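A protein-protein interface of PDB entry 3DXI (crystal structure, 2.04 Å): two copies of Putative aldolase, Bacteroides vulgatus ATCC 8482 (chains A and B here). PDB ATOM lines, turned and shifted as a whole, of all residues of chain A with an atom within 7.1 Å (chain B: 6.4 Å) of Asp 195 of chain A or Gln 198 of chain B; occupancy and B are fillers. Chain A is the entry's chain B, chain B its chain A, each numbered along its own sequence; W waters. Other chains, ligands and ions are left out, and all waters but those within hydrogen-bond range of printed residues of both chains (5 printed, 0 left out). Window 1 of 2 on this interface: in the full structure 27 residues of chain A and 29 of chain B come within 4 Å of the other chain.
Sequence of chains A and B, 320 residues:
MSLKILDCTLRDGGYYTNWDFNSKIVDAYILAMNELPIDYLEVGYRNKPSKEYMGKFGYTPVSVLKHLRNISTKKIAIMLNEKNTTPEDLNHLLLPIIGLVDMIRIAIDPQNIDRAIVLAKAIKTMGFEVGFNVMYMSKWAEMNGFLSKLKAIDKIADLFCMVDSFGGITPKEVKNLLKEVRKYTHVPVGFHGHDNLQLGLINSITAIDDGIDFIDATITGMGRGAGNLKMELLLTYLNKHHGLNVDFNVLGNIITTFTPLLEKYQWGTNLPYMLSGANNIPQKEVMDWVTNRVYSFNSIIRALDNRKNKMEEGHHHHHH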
ATOM      1  N   ASP A 164      -4.074  10.053  13.651  1.00  0.00           N
ATOM      2  CA  ASP A 164      -4.315  11.482  13.516  1.00  0.00           C
ATOM      3  C   ASP A 164      -3.168  12.148  14.274  1.00  0.00           C
ATOM      4  O   ASP A 164      -3.358  12.773  15.315  1.00  0.00           O
ATOM      5  CB  ASP A 164      -5.674  11.807  14.139  1.00  0.00           C
ATOM      6  CG  ASP A 164      -5.950  13.294  14.220  1.00  0.00           C
ATOM      7  OD1 ASP A 164      -5.376  14.058  13.416  1.00  0.00           O
ATOM      8  OD2 ASP A 164      -6.759  13.693  15.085  1.00  0.00           O
ATOM      9  N   PHE A 166      -1.331  14.854  14.149  1.00  0.00           N
ATOM     10  CA  PHE A 166      -1.302  16.244  14.587  1.00  0.00           C
ATOM     11  C   PHE A 166      -2.537  16.684  15.366  1.00  0.00           C
ATOM     12  O   PHE A 166      -2.522  17.733  16.022  1.00  0.00           O
ATOM     13  CB  PHE A 166      -1.119  17.159  13.374  1.00  0.00           C
ATOM     14  CG  PHE A 166       0.072  16.811  12.522  1.00  0.00           C
ATOM     15  CD1 PHE A 166       1.358  16.823  13.053  1.00  0.00           C
ATOM     16  CD2 PHE A 166      -0.093  16.477  11.182  1.00  0.00           C
ATOM     17  CE1 PHE A 166       2.467  16.504  12.263  1.00  0.00           C
ATOM     18  CE2 PHE A 166       1.011  16.155  10.381  1.00  0.00           C
ATOM     19  CZ  PHE A 166       2.289  16.169  10.921  1.00  0.00           C
ATOM     20  N   GLY A 167      -3.602  15.890  15.294  1.00  0.00           N
ATOM     21  CA  GLY A 167      -4.820  16.252  15.987  1.00  0.00           C
ATOM     22  C   GLY A 167      -5.559  17.330  15.217  1.00  0.00           C
ATOM     23  O   GLY A 167      -6.251  18.156  15.810  1.00  0.00           O
ATOM     24  N   GLY A 168      -5.411  17.315  13.891  1.00  0.00           N
ATOM     25  CA  GLY A 168      -6.071  18.299  13.049  1.00  0.00           C
ATOM     26  C   GLY A 168      -6.986  17.712  11.984  1.00  0.00           C
ATOM     27  O   GLY A 168      -7.668  18.450  11.277  1.00  0.00           O
ATOM     28  N   GLY A 193      -7.346   8.901  17.036  1.00  0.00           N
ATOM     29  CA  GLY A 193      -7.375  10.348  16.955  1.00  0.00           C
ATOM     30  C   GLY A 193      -6.714  11.073  18.107  1.00  0.00           C
ATOM     31  O   GLY A 193      -6.495  10.502  19.176  1.00  0.00           O
ATOM     32  N   HIS A 194      -6.370  12.338  17.872  1.00  0.00           N
ATOM     33  CA  HIS A 194      -5.777  13.178  18.902  1.00  0.00           C
ATOM     34  C   HIS A 194      -6.780  14.296  19.159  1.00  0.00           C
ATOM     35  O   HIS A 194      -7.563  14.645  18.277  1.00  0.00           O
ATOM     36  CB  HIS A 194      -4.420  13.717  18.446  1.00  0.00           C
ATOM     37  CG  HIS A 194      -3.312  12.719  18.577  1.00  0.00           C
ATOM     38  ND1 HIS A 194      -2.044  12.937  18.081  1.00  0.00           N
ATOM     39  CD2 HIS A 194      -3.287  11.487  19.137  1.00  0.00           C
ATOM     40  CE1 HIS A 194      -1.288  11.881  18.326  1.00  0.00           C
ATOM     41  NE2 HIS A 194      -2.019  10.985  18.966  1.00  0.00           N
ATOM     42  N   ASP A 195      -6.755  14.857  20.362  1.00  0.00           N
ATOM     43  CA  ASP A 195      -7.725  15.875  20.741  1.00  0.00           C
ATOM     44  C   ASP A 195      -7.330  17.344  20.652  1.00  0.00           C
ATOM     45  O   ASP A 195      -7.959  18.182  21.297  1.00  0.00           O
ATOM     46  CB  ASP A 195      -8.222  15.572  22.157  1.00  0.00           C
ATOM     47  CG  ASP A 195      -9.730  15.426  22.221  1.00  0.00           C
ATOM     48  OD1 ASP A 195     -10.338  15.167  21.158  1.00  0.00           O
ATOM     49  OD2 ASP A 195     -10.301  15.566  23.326  1.00  0.00           O
ATOM     50  N   ASN A 196      -6.316  17.664  19.853  1.00  0.00           N
ATOM     51  CA  ASN A 196      -5.870  19.050  19.714  1.00  0.00           C
ATOM     52  C   ASN A 196      -7.023  20.017  19.432  1.00  0.00           C
ATOM     53  O   ASN A 196      -7.058  21.129  19.971  1.00  0.00           O
ATOM     54  CB  ASN A 196      -4.817  19.151  18.606  1.00  0.00           C
ATOM     55  CG  ASN A 196      -3.516  18.456  18.976  1.00  0.00           C
ATOM     56  OD1 ASN A 196      -2.474  19.103  19.154  1.00  0.00           O
ATOM     57  ND2 ASN A 196      -3.568  17.134  19.109  1.00  0.00           N
ATOM     58  N   LEU A 197      -7.963  19.593  18.588  1.00  0.00           N
ATOM     59  CA  LEU A 197      -9.123  20.420  18.245  1.00  0.00           C
ATOM     60  C   LEU A 197     -10.384  19.791  18.843  1.00  0.00           C
ATOM     61  O   LEU A 197     -11.512  20.165  18.501  1.00  0.00           O
ATOM     62  CB  LEU A 197      -9.271  20.533  16.717  1.00  0.00           C
ATOM     63  CG  LEU A 197      -8.146  21.236  15.948  1.00  0.00           C
ATOM     64  CD1 LEU A 197      -8.403  21.125  14.450  1.00  0.00           C
ATOM     65  CD2 LEU A 197      -8.055  22.702  16.372  1.00  0.00           C
ATOM     66  N   GLN A 198     -10.172  18.829  19.733  1.00  0.00           N
ATOM     67  CA  GLN A 198     -11.257  18.117  20.394  1.00  0.00           C
ATOM     68  C   GLN A 198     -12.193  17.451  19.386  1.00  0.00           C
ATOM     69  O   GLN A 198     -13.407  17.401  19.587  1.00  0.00           O
ATOM     70  CB  GLN A 198     -12.054  19.072  21.285  1.00  0.00           C
ATOM     71  CG  GLN A 198     -11.203  19.871  22.253  1.00  0.00           C
ATOM     72  CD  GLN A 198     -12.035  20.612  23.282  1.00  0.00           C
ATOM     73  OE1 GLN A 198     -13.072  21.201  22.957  1.00  0.00           O
ATOM     74  NE2 GLN A 198     -11.583  20.592  24.526  1.00  0.00           N
ATOM     75  N   LEU A 199     -11.624  16.946  18.297  1.00  0.00           N
ATOM     76  CA  LEU A 199     -12.418  16.270  17.282  1.00  0.00           C
ATOM     77  C   LEU A 199     -12.314  14.752  17.429  1.00  0.00           C
ATOM     78  O   LEU A 199     -12.857  14.002  16.618  1.00  0.00           O
ATOM     79  CB  LEU A 199     -11.973  16.697  15.879  1.00  0.00           C
ATOM     80  CG  LEU A 199     -12.216  18.170  15.531  1.00  0.00           C
ATOM     81  CD1 LEU A 199     -11.779  18.426  14.093  1.00  0.00           C
ATOM     82  CD2 LEU A 199     -13.697  18.521  15.721  1.00  0.00           C
ATOM     83  N   GLY A 200     -11.619  14.306  18.472  1.00  0.00           N
ATOM     84  CA  GLY A 200     -11.464  12.882  18.700  1.00  0.00           C
ATOM     85  C   GLY A 200     -12.767  12.100  18.671  1.00  0.00           C
ATOM     86  O   GLY A 200     -12.879  11.110  17.950  1.00  0.00           O
ATOM     87  N   LEU A 201     -13.761  12.535  19.444  1.00  0.00           N
ATOM     88  CA  LEU A 201     -15.038  11.822  19.470  1.00  0.00           C
ATOM     89  C   LEU A 201     -15.763  11.804  18.131  1.00  0.00           C
ATOM     90  O   LEU A 201     -16.059  10.735  17.608  1.00  0.00           O
ATOM     91  CB  LEU A 201     -15.982  12.403  20.531  1.00  0.00           C
ATOM     92  CG  LEU A 201     -17.368  11.741  20.527  1.00  0.00           C
ATOM     93  CD1 LEU A 201     -17.246  10.261  20.900  1.00  0.00           C
ATOM     94  CD2 LEU A 201     -18.282  12.462  21.498  1.00  0.00           C
ATOM     95  N   ILE A 202     -16.053  12.977  17.572  1.00  0.00           N
ATOM     96  CA  ILE A 202     -16.781  13.030  16.300  1.00  0.00           C
ATOM     97  C   ILE A 202     -16.052  12.307  15.166  1.00  0.00           C
ATOM     98  O   ILE A 202     -16.691  11.677  14.320  1.00  0.00           O
ATOM     99  CB  ILE A 202     -17.102  14.497  15.880  1.00  0.00           C
ATOM    100  CG1 ILE A 202     -18.109  14.491  14.734  1.00  0.00           C
ATOM    101  CG2 ILE A 202     -15.833  15.238  15.468  1.00  0.00           C
ATOM    102  CD1 ILE A 202     -19.421  13.823  15.106  1.00  0.00           C
ATOM    103  N   GLY A 221      -8.198  10.548  28.330  1.00  0.00           N
ATOM    104  CA  GLY A 221      -7.477  11.008  27.157  1.00  0.00           C
ATOM    105  C   GLY A 221      -5.991  11.155  27.411  1.00  0.00           C
ATOM    106  O   GLY A 221      -5.280  11.792  26.633  1.00  0.00           O
ATOM    107  N   ALA A 226      -1.899  17.451  23.807  1.00  0.00           N
ATOM    108  CA  ALA A 226      -3.357  17.519  23.778  1.00  0.00           C
ATOM    109  C   ALA A 226      -3.995  16.195  24.174  1.00  0.00           C
ATOM    110  O   ALA A 226      -5.128  16.168  24.633  1.00  0.00           O
ATOM    111  CB  ALA A 226      -3.838  17.934  22.395  1.00  0.00           C
ATOM    112  N   GLY A 227      -3.269  15.100  23.986  1.00  0.00           N
ATOM    113  CA  GLY A 227      -3.808  13.810  24.363  1.00  0.00           C
ATOM    114  C   GLY A 227      -4.653  13.126  23.306  1.00  0.00           C
ATOM    115  O   GLY A 227      -4.690  13.549  22.148  1.00  0.00           O
ATOM    116  N   ASN A 228      -5.344  12.069  23.722  1.00  0.00           N
ATOM    117  CA  ASN A 228      -6.176  11.270  22.825  1.00  0.00           C
ATOM    118  C   ASN A 228      -7.665  11.391  23.113  1.00  0.00           C
ATOM    119  O   ASN A 228      -8.093  12.199  23.928  1.00  0.00           O
ATOM    120  CB  ASN A 228      -5.801   9.794  22.952  1.00  0.00           C
ATOM    121  CG  ASN A 228      -4.325   9.556  22.800  1.00  0.00           C
ATOM    122  OD1 ASN A 228      -3.654   9.104  23.736  1.00  0.00           O
ATOM    123  ND2 ASN A 228      -3.800   9.857  21.622  1.00  0.00           N
ATOM    124  N   LEU A 229      -8.447  10.564  22.428  1.00  0.00           N
ATOM    125  CA  LEU A 229      -9.883  10.534  22.646  1.00  0.00           C
ATOM    126  C   LEU A 229     -10.069  10.012  24.065  1.00  0.00           C
ATOM    127  O   LEU A 229      -9.396   9.060  24.462  1.00  0.00           O
ATOM    128  CB  LEU A 229     -10.550   9.572  21.660  1.00  0.00           C
ATOM    129  CG  LEU A 229     -12.005   9.184  21.936  1.00  0.00           C
ATOM    130  CD1 LEU A 229     -12.883  10.425  21.988  1.00  0.00           C
ATOM    131  CD2 LEU A 229     -12.479   8.241  20.854  1.00  0.00           C
ATOM    132  N   LYS A 230     -10.949  10.650  24.831  1.00  0.00           N
ATOM    133  CA  LYS A 230     -11.217  10.206  26.198  1.00  0.00           C
ATOM    134  C   LYS A 230     -12.082   8.957  26.106  1.00  0.00           C
ATOM    135  O   LYS A 230     -13.205   9.006  25.594  1.00  0.00           O
ATOM    136  CB  LYS A 230     -11.951  11.290  26.997  1.00  0.00           C
ATOM    137  CG  LYS A 230     -11.098  12.519  27.304  1.00  0.00           C
ATOM    138  CD  LYS A 230     -11.926  13.644  27.902  1.00  0.00           C
ATOM    139  CE  LYS A 230     -11.089  14.890  28.107  1.00  0.00           C
ATOM    140  NZ  LYS A 230     -11.929  16.056  28.500  1.00  0.00           N
ATOM    141  N   LEU A 233     -15.481   9.210  27.245  1.00  0.00           N
ATOM    142  CA  LEU A 233     -16.339   9.951  26.333  1.00  0.00           C
ATOM    143  C   LEU A 233     -16.887   9.031  25.241  1.00  0.00           C
ATOM    144  O   LEU A 233     -18.074   9.058  24.929  1.00  0.00           O
ATOM    145  CB  LEU A 233     -15.554  11.101  25.702  1.00  0.00           C
ATOM    146  CG  LEU A 233     -16.323  12.070  24.816  1.00  0.00           C
ATOM    147  CD1 LEU A 233     -17.519  12.603  25.571  1.00  0.00           C
ATOM    148  CD2 LEU A 233     -15.397  13.207  24.393  1.00  0.00           C
ATOM    149  N   GLY A 268      -4.000  17.790  27.785  1.00  0.00           N
ATOM    150  CA  GLY A 268      -5.215  18.358  27.229  1.00  0.00           C
ATOM    151  C   GLY A 268      -4.867  19.500  26.296  1.00  0.00           C
ATOM    152  O   GLY A 268      -3.822  20.126  26.443  1.00  0.00           O
ATOM    153  N   THR A 269      -5.740  19.791  25.339  1.00  0.00           N
ATOM    154  CA  THR A 269      -5.443  20.852  24.393  1.00  0.00           C
ATOM    155  C   THR A 269      -5.461  22.246  25.015  1.00  0.00           C
ATOM    156  O   THR A 269      -5.976  22.449  26.111  1.00  0.00           O
ATOM    157  CB  THR A 269      -6.408  20.820  23.188  1.00  0.00           C
ATOM    158  OG1 THR A 269      -5.813  21.537  22.099  1.00  0.00           O
ATOM    159  CG2 THR A 269      -7.744  21.465  23.538  1.00  0.00           C
ATOM    160  N   ASN A 270      -4.870  23.193  24.298  1.00  0.00           N
ATOM    161  CA  ASN A 270      -4.786  24.582  24.715  1.00  0.00           C
ATOM    162  C   ASN A 270      -4.453  25.356  23.433  1.00  0.00           C
ATOM    163  O   ASN A 270      -4.293  24.746  22.375  1.00  0.00           O
ATOM    164  CB  ASN A 270      -3.693  24.753  25.786  1.00  0.00           C
ATOM    165  CG  ASN A 270      -2.400  24.046  25.426  1.00  0.00           C
ATOM    166  OD1 ASN A 270      -1.896  24.184  24.313  1.00  0.00           O
ATOM    167  ND2 ASN A 270      -1.849  23.293  26.373  1.00  0.00           N
ATOM    168  N   TYR A 273      -1.568  24.030  21.305  1.00  0.00           N
ATOM    169  CA  TYR A 273      -1.920  22.740  20.728  1.00  0.00           C
ATOM    170  C   TYR A 273      -3.072  22.818  19.730  1.00  0.00           C
ATOM    171  O   TYR A 273      -3.204  21.953  18.868  1.00  0.00           O
ATOM    172  CB  TYR A 273      -2.208  21.731  21.858  1.00  0.00           C
ATOM    173  CG  TYR A 273      -0.970  21.396  22.674  1.00  0.00           C
ATOM    174  CD1 TYR A 273       0.299  21.457  22.096  1.00  0.00           C
ATOM    175  CD2 TYR A 273      -1.064  20.989  24.008  1.00  0.00           C
ATOM    176  CE1 TYR A 273       1.445  21.123  22.820  1.00  0.00           C
ATOM    177  CE2 TYR A 273       0.080  20.652  24.743  1.00  0.00           C
ATOM    178  CZ  TYR A 273       1.331  20.719  24.138  1.00  0.00           C
ATOM    179  OH  TYR A 273       2.468  20.372  24.833  1.00  0.00           O
ATOM    180  N   MET A 274      -3.900  23.851  19.831  1.00  0.00           N
ATOM    181  CA  MET A 274      -4.992  24.000  18.874  1.00  0.00           C
ATOM    182  C   MET A 274      -4.352  24.474  17.577  1.00  0.00           C
ATOM    183  O   MET A 274      -4.742  24.075  16.481  1.00  0.00           O
ATOM    184  CB  MET A 274      -6.005  25.047  19.356  1.00  0.00           C
ATOM    185  CG  MET A 274      -6.529  24.796  20.760  1.00  0.00           C
ATOM    186  SD  MET A 274      -7.910  26.057  21.276  1.00  0.00           S
ATOM    187  CE  MET A 274      -6.968  27.633  21.846  1.00  0.00           C
ATOM    188  N   GLN A 283       3.162  18.940  17.867  1.00  0.00           N
ATOM    189  CA  GLN A 283       2.988  19.806  19.028  1.00  0.00           C
ATOM    190  C   GLN A 283       4.257  20.195  19.765  1.00  0.00           C
ATOM    191  O   GLN A 283       4.317  21.276  20.348  1.00  0.00           O
ATOM    192  CB  GLN A 283       1.971  19.209  20.018  1.00  0.00           C
ATOM    193  CG  GLN A 283       1.813  17.706  19.974  1.00  0.00           C
ATOM    194  CD  GLN A 283       0.701  17.203  20.894  1.00  0.00           C
ATOM    195  OE1 GLN A 283      -0.384  17.789  20.972  1.00  0.00           O
ATOM    196  NE2 GLN A 283       0.966  16.099  21.584  1.00  0.00           N
ATOM    197  N   GLY B 167     -26.315  19.912  26.074  1.00  0.00           N
ATOM    198  CA  GLY B 167     -24.982  19.638  25.571  1.00  0.00           C
ATOM    199  C   GLY B 167     -24.908  18.234  24.999  1.00  0.00           C
ATOM    200  O   GLY B 167     -23.875  17.564  25.090  1.00  0.00           O
ATOM    201  N   HIS B 194     -23.268  23.566  23.909  1.00  0.00           N
ATOM    202  CA  HIS B 194     -22.619  23.292  25.183  1.00  0.00           C
ATOM    203  C   HIS B 194     -21.614  22.180  24.922  1.00  0.00           C
ATOM    204  O   HIS B 194     -21.758  21.416  23.957  1.00  0.00           O
ATOM    205  CB  HIS B 194     -23.637  22.887  26.243  1.00  0.00           C
ATOM    206  CG  HIS B 194     -24.392  24.047  26.814  1.00  0.00           C
ATOM    207  ND1 HIS B 194     -25.404  23.896  27.736  1.00  0.00           N
ATOM    208  CD2 HIS B 194     -24.276  25.377  26.597  1.00  0.00           C
ATOM    209  CE1 HIS B 194     -25.880  25.085  28.061  1.00  0.00           C
ATOM    210  NE2 HIS B 194     -25.213  26.001  27.384  1.00  0.00           N
ATOM    211  N   ASP B 195     -20.602  22.084  25.778  1.00  0.00           N
ATOM    212  CA  ASP B 195     -19.540  21.112  25.577  1.00  0.00           C
ATOM    213  C   ASP B 195     -19.579  19.827  26.396  1.00  0.00           C
ATOM    214  O   ASP B 195     -18.535  19.208  26.618  1.00  0.00           O
ATOM    215  CB  ASP B 195     -18.191  21.815  25.781  1.00  0.00           C
ATOM    216  CG  ASP B 195     -17.274  21.672  24.583  1.00  0.00           C
ATOM    217  OD1 ASP B 195     -17.791  21.568  23.450  1.00  0.00           O
ATOM    218  OD2 ASP B 195     -16.039  21.674  24.770  1.00  0.00           O
ATOM    219  N   ASN B 196     -20.765  19.408  26.831  1.00  0.00           N
ATOM    220  CA  ASN B 196     -20.867  18.183  27.620  1.00  0.00           C
ATOM    221  C   ASN B 196     -20.230  16.990  26.908  1.00  0.00           C
ATOM    222  O   ASN B 196     -19.591  16.154  27.544  1.00  0.00           O
ATOM    223  CB  ASN B 196     -22.330  17.878  27.956  1.00  0.00           C
ATOM    224  CG  ASN B 196     -22.918  18.875  28.930  1.00  0.00           C
ATOM    225  OD1 ASN B 196     -23.289  18.523  30.054  1.00  0.00           O
ATOM    226  ND2 ASN B 196     -22.995  20.133  28.510  1.00  0.00           N
ATOM    227  N   LEU B 197     -20.401  16.914  25.591  1.00  0.00           N
ATOM    228  CA  LEU B 197     -19.831  15.820  24.798  1.00  0.00           C
ATOM    229  C   LEU B 197     -18.711  16.321  23.893  1.00  0.00           C
ATOM    230  O   LEU B 197     -18.247  15.605  23.001  1.00  0.00           O
ATOM    231  CB  LEU B 197     -20.913  15.165  23.937  1.00  0.00           C
ATOM    232  CG  LEU B 197     -21.991  14.385  24.692  1.00  0.00           C
ATOM    233  CD1 LEU B 197     -23.035  13.850  23.705  1.00  0.00           C
ATOM    234  CD2 LEU B 197     -21.336  13.242  25.472  1.00  0.00           C
ATOM    235  N   GLN B 198     -18.283  17.555  24.132  1.00  0.00           N
ATOM    236  CA  GLN B 198     -17.241  18.189  23.337  1.00  0.00           C
ATOM    237  C   GLN B 198     -17.590  18.248  21.846  1.00  0.00           C
ATOM    238  O   GLN B 198     -16.723  18.118  20.980  1.00  0.00           O
ATOM    239  CB  GLN B 198     -15.895  17.491  23.558  1.00  0.00           C
ATOM    240  CG  GLN B 198     -15.290  17.797  24.932  1.00  0.00           C
ATOM    241  CD  GLN B 198     -13.913  17.194  25.126  1.00  0.00           C
ATOM    242  OE1 GLN B 198     -13.309  16.686  24.183  1.00  0.00           O
ATOM    243  NE2 GLN B 198     -13.400  17.265  26.346  1.00  0.00           N
ATOM    244  N   LEU B 199     -18.874  18.447  21.555  1.00  0.00           N
ATOM    245  CA  LEU B 199     -19.332  18.560  20.174  1.00  0.00           C
ATOM    246  C   LEU B 199     -19.608  20.034  19.840  1.00  0.00           C
ATOM    247  O   LEU B 199     -20.120  20.356  18.766  1.00  0.00           O
ATOM    248  CB  LEU B 199     -20.602  17.730  19.956  1.00  0.00           C
ATOM    249  CG  LEU B 199     -20.480  16.199  20.033  1.00  0.00           C
ATOM    250  CD1 LEU B 199     -21.857  15.560  19.814  1.00  0.00           C
ATOM    251  CD2 LEU B 199     -19.491  15.709  18.979  1.00  0.00           C
ATOM    252  N   GLY B 200     -19.263  20.923  20.767  1.00  0.00           N
ATOM    253  CA  GLY B 200     -19.482  22.339  20.541  1.00  0.00           C
ATOM    254  C   GLY B 200     -18.867  22.845  19.245  1.00  0.00           C
ATOM    255  O   GLY B 200     -19.534  23.512  18.457  1.00  0.00           O
ATOM    256  N   LEU B 201     -17.594  22.535  19.013  1.00  0.00           N
ATOM    257  CA  LEU B 201     -16.934  22.996  17.798  1.00  0.00           C
ATOM    258  C   LEU B 201     -17.545  22.403  16.535  1.00  0.00           C
ATOM    259  O   LEU B 201     -17.955  23.140  15.640  1.00  0.00           O
ATOM    260  CB  LEU B 201     -15.433  22.671  17.823  1.00  0.00           C
ATOM    261  CG  LEU B 201     -14.668  23.038  16.539  1.00  0.00           C
ATOM    262  CD1 LEU B 201     -14.636  24.551  16.351  1.00  0.00           C
ATOM    263  CD2 LEU B 201     -13.259  22.484  16.606  1.00  0.00           C
ATOM    264  N   ILE B 202     -17.621  21.078  16.455  1.00  0.00           N
ATOM    265  CA  ILE B 202     -18.159  20.464  15.251  1.00  0.00           C
ATOM    266  C   ILE B 202     -19.620  20.816  14.976  1.00  0.00           C
ATOM    267  O   ILE B 202     -20.013  20.949  13.816  1.00  0.00           O
ATOM    268  CB  ILE B 202     -17.959  18.914  15.244  1.00  0.00           C
ATOM    269  CG1 ILE B 202     -18.232  18.385  13.836  1.00  0.00           C
ATOM    270  CG2 ILE B 202     -18.868  18.238  16.264  1.00  0.00           C
ATOM    271  CD1 ILE B 202     -17.390  19.085  12.748  1.00  0.00           C
ATOM    272  N   LYS B 230     -15.449  26.713  23.271  1.00  0.00           N
ATOM    273  CA  LYS B 230     -14.329  27.603  23.566  1.00  0.00           C
ATOM    274  C   LYS B 230     -14.102  28.531  22.376  1.00  0.00           C
ATOM    275  O   LYS B 230     -13.802  28.076  21.264  1.00  0.00           O
ATOM    276  CB  LYS B 230     -13.062  26.789  23.868  1.00  0.00           C
ATOM    277  CG  LYS B 230     -13.200  25.937  25.122  1.00  0.00           C
ATOM    278  CD  LYS B 230     -11.880  25.340  25.580  1.00  0.00           C
ATOM    279  CE  LYS B 230     -11.490  24.129  24.765  1.00  0.00           C
ATOM    280  NZ  LYS B 230     -10.918  23.093  25.669  1.00  0.00           N
ATOM    281  N   THR B 269     -16.196  19.541  30.841  1.00  0.00           N
ATOM    282  CA  THR B 269     -16.967  18.312  30.989  1.00  0.00           C
ATOM    283  C   THR B 269     -16.238  17.237  31.800  1.00  0.00           C
ATOM    284  O   THR B 269     -15.030  17.310  32.012  1.00  0.00           O
ATOM    285  CB  THR B 269     -17.346  17.731  29.604  1.00  0.00           C
ATOM    286  OG1 THR B 269     -18.325  16.702  29.773  1.00  0.00           O
ATOM    287  CG2 THR B 269     -16.118  17.130  28.915  1.00  0.00           C
ATOM    288  N   MET B 274     -20.956  14.259  31.036  1.00  0.00           N
ATOM    289  CA  MET B 274     -21.055  13.541  29.768  1.00  0.00           C
ATOM    290  C   MET B 274     -22.367  12.765  29.807  1.00  0.00           C
ATOM    291  O   MET B 274     -23.099  12.703  28.816  1.00  0.00           O
ATOM    292  CB  MET B 274     -19.902  12.544  29.603  1.00  0.00           C
ATOM    293  CG  MET B 274     -18.557  13.180  29.284  1.00  0.00           C
ATOM    294  SD  MET B 274     -17.085  11.946  29.465  1.00  0.00           S
ATOM    295  CE  MET B 274     -15.658  13.198  29.856  1.00  0.00           C
HETATM  296  O   HOH W   1      -8.191  24.441  26.205  1.00  0.00           O
HETATM  297  O   HOH W   2     -11.831  13.540  24.064  1.00  0.00           O
HETATM  298  O   HOH W   3     -14.867  23.715  23.176  1.00  0.00           O
HETATM  299  O   HOH W   4     -13.122  15.148  31.015  1.00  0.00           O
HETATM  300  O   HOH W   5     -15.998  21.769  21.213  1.00  0.00           O
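The side-chain amide oxygen (OE1) of Gln 198 of chain B sits close to the side-chain carboxylate (OD2) of Asp 195 of chain A (3.3 Å).
The side-chain amide nitrogen (NE2) of Gln 198 of chain B lies close to the side-chain amino group (NZ) of Lys 230 of chain A (2.9 Å).
The side-chain amide nitrogen (NE2) of Gln 198 of chain A sits close to the side-chain amino group (NZ) of Lys 230 of chain B (2.8 Å).
N of Asp 195 of chain A lies within hydrogen-bond range of O of Gly 227 of chain A (3.0 Å).
The backbone NH (N) of Gly 200 of chain B lies within hydrogen-bond range of the side-chain carboxylate (OD1) of Asp 195 of chain B, 3.1 Å away.
The side-chain carboxylate (OD1) of Asp 195 of chain A is in hydrogen-bond range of the backbone NH (N) of Gly 200 of chain A.
Leu 197 of chain A touches Leu 201 of chain B (O to CD2, 3.5 Å).
Gln 198 of chain A touches Asp 195 of chain B (OE1 to OD2, 3.5 Å).
O of Gln 198 of chain B touches O of Gln 198 of chain A (3.7 Å).
Leu 197 of chain B touches Leu 201 of chain A.
CG1 of Ile 202 of chain A touches CG1 of Ile 202 of chain B, 3.998 Å away.
Leu 197 of chain B touches Leu 233 of chain A.
CA of Leu 233 of chain A touches SD of Met 274 of chain B, 3.8 Å away.
Of the printed residues of chain B, Asp 195 of chain A touches Gln 198.
Printed residues of chain B within 4 Å of Ile 202 of chain A: Ile 202.
Gly 167 of chain B touches none of the printed residues of chain A.
His 194 of chain B touches none of the printed residues of chain A.
Gln 198 of chain B touches just these residues of chain A: Asp 195 (3.3 Å), Gln 198 (3.7 Å) and Lys 230 (2.9 Å).
Printed residues of chain A within 4 Å of Met 274 of chain B: Leu 233.
Printed residues of chain A that touch a printed residue of chain B: Asp 195, Leu 197, Gln 198, Leu 201, Ile 202, Lys 230 and Leu 233.
Hydrophobic or aromatic side chains of chain A within 4 Å of the printed part of chain B: Leu 201, Ile 202 and Leu 233.
Along chain A the printed residues that touch a printed residue of chain B span positions 195 to 233.
Of the 13 printed residues of chain B, 7 touch a printed residue of chain A.
Asp 195 of chain A touches Gln 198 of chain B, and with the chains exchanged Gln 198 of chain A touches Asp 195 of chain B.
Leu 197 of chain A touches Leu 201 of chain B, and with the chains exchanged Leu 201 of chain A touches Leu 197 of chain B.
Gln 198 of chain A touches Lys 230 of chain B, and with the chains exchanged Lys 230 of chain A touches Gln 198 of chain B.
Of the 10 pairs that touch across the chains among the printed residues, 8 have their exchanged pair printed and touching as well.
Water W2 lies within hydrogen-bond range of OD2 of Asp 195 of chain A (2.6 Å), N of Lys 230 of chain A (3.1 Å) and OE1 of Gln 198 of chain B (3.5 Å).
Water W3 lies within hydrogen-bond range of the side-chain carboxylate (OD2) of Asp 195 of chain B (2.8 Å), the backbone NH (N) of Lys 230 of chain B (3.1 Å) and the side-chain amide oxygen (OE1) of Gln 198 of chain A (3.1 Å).
Water W1 bridges O of Thr 269 of chain A and NZ of Lys 230 of chain B.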
